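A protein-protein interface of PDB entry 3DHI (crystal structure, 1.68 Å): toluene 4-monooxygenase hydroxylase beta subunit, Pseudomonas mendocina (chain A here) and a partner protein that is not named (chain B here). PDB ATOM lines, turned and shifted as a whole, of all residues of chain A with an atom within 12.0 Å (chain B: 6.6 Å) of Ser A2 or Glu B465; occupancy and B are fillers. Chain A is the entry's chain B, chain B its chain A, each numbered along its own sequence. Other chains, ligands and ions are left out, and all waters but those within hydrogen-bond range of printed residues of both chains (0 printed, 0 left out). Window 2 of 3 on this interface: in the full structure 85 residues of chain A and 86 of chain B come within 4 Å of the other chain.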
ATOM      1  N   SER A   2      16.138  -8.953  19.390  1.00  0.00           N
ATOM      2  CA  SER A   2      15.659  -7.548  19.498  1.00  0.00           C
ATOM      3  C   SER A   2      14.735  -7.164  18.337  1.00  0.00           C
ATOM      4  O   SER A   2      13.507  -7.113  18.504  1.00  0.00           O
ATOM      5  CB  SER A   2      16.843  -6.584  19.581  1.00  0.00           C
ATOM      6  OG  SER A   2      16.399  -5.264  19.839  1.00  0.00           O
ATOM      7  N   PHE A   3      15.333  -6.902  17.172  1.00  0.00           N
ATOM      8  CA  PHE A   3      14.615  -6.414  15.976  1.00  0.00           C
ATOM      9  C   PHE A   3      13.888  -5.077  16.154  1.00  0.00           C
ATOM     10  O   PHE A   3      13.134  -4.865  17.115  1.00  0.00           O
ATOM     11  CB  PHE A   3      13.655  -7.465  15.403  1.00  0.00           C
ATOM     12  CG  PHE A   3      14.274  -8.347  14.360  1.00  0.00           C
ATOM     13  CD1 PHE A   3      14.420  -9.713  14.584  1.00  0.00           C
ATOM     14  CD2 PHE A   3      14.717  -7.809  13.150  1.00  0.00           C
ATOM     15  CE1 PHE A   3      14.992 -10.533  13.614  1.00  0.00           C
ATOM     16  CE2 PHE A   3      15.293  -8.622  12.177  1.00  0.00           C
ATOM     17  CZ  PHE A   3      15.428  -9.987  12.409  1.00  0.00           C
ATOM     18  N   GLU A   4      14.114  -4.191  15.191  1.00  0.00           N
ATOM     19  CA  GLU A   4      13.523  -2.861  15.206  1.00  0.00           C
ATOM     20  C   GLU A   4      12.077  -2.827  14.731  1.00  0.00           C
ATOM     21  O   GLU A   4      11.603  -3.750  14.064  1.00  0.00           O
ATOM     22  CB  GLU A   4      14.344  -1.918  14.338  1.00  0.00           C
ATOM     23  CG  GLU A   4      15.797  -1.876  14.721  1.00  0.00           C
ATOM     24  CD  GLU A   4      16.557  -0.832  13.951  1.00  0.00           C
ATOM     25  OE1 GLU A   4      17.727  -1.089  13.598  1.00  0.00           O
ATOM     26  OE2 GLU A   4      15.981   0.246  13.698  1.00  0.00           O
ATOM     27  N   SER A   5      11.385  -1.756  15.119  1.00  0.00           N
ATOM     28  CA  SER A   5      10.163  -1.329  14.470  1.00  0.00           C
ATOM     29  C   SER A   5      10.547  -0.124  13.605  1.00  0.00           C
ATOM     30  O   SER A   5      11.020   0.890  14.122  1.00  0.00           O
ATOM     31  CB  SER A   5       9.100  -0.972  15.516  1.00  0.00           C
ATOM     32  OG  SER A   5       8.456  -2.139  16.045  1.00  0.00           O
ATOM     33  N   LYS A   6      10.392  -0.254  12.286  1.00  0.00           N
ATOM     34  CA  LYS A   6      10.782   0.807  11.344  1.00  0.00           C
ATOM     35  C   LYS A   6       9.586   1.226  10.500  1.00  0.00           C
ATOM     36  O   LYS A   6       8.665   0.436  10.291  1.00  0.00           O
ATOM     37  CB  LYS A   6      11.893   0.344  10.402  1.00  0.00           C
ATOM     38  CG  LYS A   6      13.273   0.209  11.014  1.00  0.00           C
ATOM     39  CD  LYS A   6      14.300   0.137   9.895  1.00  0.00           C
ATOM     40  CE  LYS A   6      15.665  -0.318  10.395  1.00  0.00           C
ATOM     41  NZ  LYS A   6      16.689  -0.235   9.310  1.00  0.00           N
ATOM     42  N   PRO B 461      24.364 -15.000  14.596  1.00  0.00           N
ATOM     43  CA  PRO B 461      24.357 -16.124  15.558  1.00  0.00           C
ATOM     44  C   PRO B 461      23.366 -17.264  15.211  1.00  0.00           C
ATOM     45  O   PRO B 461      22.574 -17.127  14.277  1.00  0.00           O
ATOM     46  CB  PRO B 461      23.976 -15.450  16.877  1.00  0.00           C
ATOM     47  CG  PRO B 461      23.161 -14.265  16.476  1.00  0.00           C
ATOM     48  CD  PRO B 461      23.720 -13.797  15.156  1.00  0.00           C
ATOM     49  N   MET B 462      23.415 -18.369  15.965  1.00  0.00           N
ATOM     50  CA  MET B 462      22.609 -19.569  15.659  1.00  0.00           C
ATOM     51  C   MET B 462      21.287 -19.606  16.418  1.00  0.00           C
ATOM     52  O   MET B 462      21.047 -20.481  17.261  1.00  0.00           O
ATOM     53  CB  MET B 462      23.413 -20.842  15.910  1.00  0.00           C
ATOM     54  CG  MET B 462      24.416 -21.172  14.802  1.00  0.00           C
ATOM     55  SD  MET B 462      25.471 -22.609  15.142  1.00  0.00           S
ATOM     56  CE  MET B 462      24.426 -23.989  14.689  1.00  0.00           C
ATOM     57  N   THR B 463      20.422 -18.654  16.096  1.00  0.00           N
ATOM     58  CA  THR B 463      19.165 -18.449  16.806  1.00  0.00           C
ATOM     59  C   THR B 463      18.125 -18.101  15.759  1.00  0.00           C
ATOM     60  O   THR B 463      18.493 -17.828  14.616  1.00  0.00           O
ATOM     61  CB  THR B 463      19.286 -17.253  17.770  1.00  0.00           C
ATOM     62  OG1 THR B 463      19.787 -16.117  17.048  1.00  0.00           O
ATOM     63  CG2 THR B 463      20.251 -17.571  18.915  1.00  0.00           C
ATOM     64  N   LEU B 464      16.845 -18.086  16.142  1.00  0.00           N
ATOM     65  CA  LEU B 464      15.793 -17.601  15.241  1.00  0.00           C
ATOM     66  C   LEU B 464      16.217 -16.227  14.709  1.00  0.00           C
ATOM     67  O   LEU B 464      16.321 -16.019  13.487  1.00  0.00           O
ATOM     68  CB  LEU B 464      14.429 -17.527  15.955  1.00  0.00           C
ATOM     69  CG  LEU B 464      13.174 -17.066  15.183  1.00  0.00           C
ATOM     70  CD1 LEU B 464      12.938 -17.874  13.903  1.00  0.00           C
ATOM     71  CD2 LEU B 464      11.927 -17.108  16.060  1.00  0.00           C
ATOM     72  N   GLU B 465      16.512 -15.317  15.638  1.00  0.00           N
ATOM     73  CA  GLU B 465      16.975 -13.981  15.298  1.00  0.00           C
ATOM     74  C   GLU B 465      18.157 -13.962  14.331  1.00  0.00           C
ATOM     75  O   GLU B 465      18.134 -13.219  13.350  1.00  0.00           O
ATOM     76  CB  GLU B 465      17.319 -13.184  16.554  1.00  0.00           C
ATOM     77  CG  GLU B 465      17.721 -11.767  16.227  1.00  0.00           C
ATOM     78  CD  GLU B 465      17.647 -10.828  17.405  1.00  0.00           C
ATOM     79  OE1 GLU B 465      18.330  -9.784  17.360  1.00  0.00           O
ATOM     80  OE2 GLU B 465      16.911 -11.119  18.369  1.00  0.00           O
ATOM     81  N   GLY B 466      19.186 -14.763  14.610  1.00  0.00           N
ATOM     82  CA  GLY B 466      20.361 -14.844  13.744  1.00  0.00           C
ATOM     83  C   GLY B 466      19.998 -15.248  12.319  1.00  0.00           C
ATOM     84  O   GLY B 466      20.485 -14.665  11.357  1.00  0.00           O
ATOM     85  N   ALA B 467      19.149 -16.268  12.204  1.00  0.00           N
ATOM     86  CA  ALA B 467      18.665 -16.745  10.905  1.00  0.00           C
ATOM     87  C   ALA B 467      17.834 -15.686  10.179  1.00  0.00           C
ATOM     88  O   ALA B 467      18.003 -15.482   8.972  1.00  0.00           O
ATOM     89  CB  ALA B 467      17.841 -18.049  11.081  1.00  0.00           C
ATOM     90  N   LEU B 468      16.936 -15.039  10.916  1.00  0.00           N
ATOM     91  CA  LEU B 468      16.059 -14.000  10.364  1.00  0.00           C
ATOM     92  C   LEU B 468      16.854 -12.844   9.816  1.00  0.00           C
ATOM     93  O   LEU B 468      16.569 -12.353   8.721  1.00  0.00           O
ATOM     94  CB  LEU B 468      15.057 -13.501  11.406  1.00  0.00           C
ATOM     95  CG  LEU B 468      13.864 -14.401  11.728  1.00  0.00           C
ATOM     96  CD1 LEU B 468      13.165 -13.918  12.982  1.00  0.00           C
ATOM     97  CD2 LEU B 468      12.884 -14.478  10.558  1.00  0.00           C
ATOM     98  N   LYS B 469      17.862 -12.409  10.574  1.00  0.00           N
ATOM     99  CA  LYS B 469      18.773 -11.388  10.090  1.00  0.00           C
ATOM    100  C   LYS B 469      19.570 -11.856   8.876  1.00  0.00           C
ATOM    101  O   LYS B 469      19.730 -11.103   7.915  1.00  0.00           O
ATOM    102  CB  LYS B 469      19.678 -10.906  11.228  1.00  0.00           C
ATOM    103  CG  LYS B 469      18.893 -10.100  12.276  1.00  0.00           C
ATOM    104  CD  LYS B 469      19.778  -9.617  13.438  1.00  0.00           C
ATOM    105  CE  LYS B 469      19.120  -8.501  14.238  1.00  0.00           C
ATOM    106  NZ  LYS B 469      17.697  -8.798  14.593  1.00  0.00           N
ATOM    107  N   TYR B 470      20.054 -13.101   8.906  1.00  0.00           N
ATOM    108  CA  TYR B 470      20.781 -13.674   7.769  1.00  0.00           C
ATOM    109  C   TYR B 470      19.894 -13.648   6.500  1.00  0.00           C
ATOM    110  O   TYR B 470      20.378 -13.431   5.393  1.00  0.00           O
ATOM    111  CB  TYR B 470      21.212 -15.115   8.090  1.00  0.00           C
ATOM    112  CG  TYR B 470      21.765 -15.859   6.897  1.00  0.00           C
ATOM    113  CD1 TYR B 470      23.082 -15.703   6.504  1.00  0.00           C
ATOM    114  CD2 TYR B 470      20.951 -16.735   6.158  1.00  0.00           C
ATOM    115  CE1 TYR B 470      23.591 -16.368   5.399  1.00  0.00           C
ATOM    116  CE2 TYR B 470      21.450 -17.407   5.057  1.00  0.00           C
ATOM    117  CZ  TYR B 470      22.766 -17.221   4.676  1.00  0.00           C
ATOM    118  OH  TYR B 470      23.302 -17.873   3.597  1.00  0.00           O
ATOM    119  N   ILE B 476      10.730  -5.674  12.583  1.00  0.00           N
ATOM    120  CA  ILE B 476       9.537  -6.411  13.021  1.00  0.00           C
ATOM    121  C   ILE B 476       8.450  -6.415  11.940  1.00  0.00           C
ATOM    122  O   ILE B 476       7.817  -7.439  11.687  1.00  0.00           O
ATOM    123  CB  ILE B 476       8.972  -5.774  14.351  1.00  0.00           C
ATOM    124  CG1 ILE B 476       9.970  -5.956  15.504  1.00  0.00           C
ATOM    125  CG2 ILE B 476       7.594  -6.335  14.735  1.00  0.00           C
ATOM    126  CD1 ILE B 476       9.588  -5.203  16.802  1.00  0.00           C
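O of Glu A4 lies within hydrogen-bond range of N of Ile B476 (2.6 Å).
The backbone NH of Ser A2 lies within hydrogen-bond range of the side-chain carboxylate of Glu B465, at 2.5 Å.
OE1 of Glu B465 lies within salt-bridge range of NZ of Lys B469, 3.0 Å away.
CG of Glu B465 touches CE1 of Phe A3 (3.97 Å).
Phe A3 touches Leu B468 (CZ to CB, 3.7 Å).
Lys B469 touches Phe A3 (NZ to CE1, 3.4 Å).
Phe A3 touches Ile B476 (O to CD1, 3.6 Å).
Ser A5 touches Ile B476.
Printed residues of chain A within 4 Å of Glu B465: Ser A2 (2.5 Å) and Phe A3 (3.97 Å).
No residue of chain A comes within 4 Å of Leu B464.
No residue of chain A comes within 4 Å of Gly B466.
Of chain A, only Phe A3 (3.7 Å) comes within 4 Å of Leu B468.
Of the printed residues of chain B, Phe A3 touches Glu B465 (3.97 Å), Leu B468 (3.7 Å), Lys B469 (3.4 Å) and Ile B476 (3.6 Å).
Of the printed residues of chain A, Ile B476 touches Phe A3 (3.6 Å), Glu A4 (2.6 Å) and Ser A5 (3.4 Å).
Lys A6 touches none of the printed residues of chain B.
Hydrophobic or aromatic side chains of chain B that line the printed part of chain A: Leu B468 and Ile B476.
Among the printed residues, 7 pairs touch across the chains.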
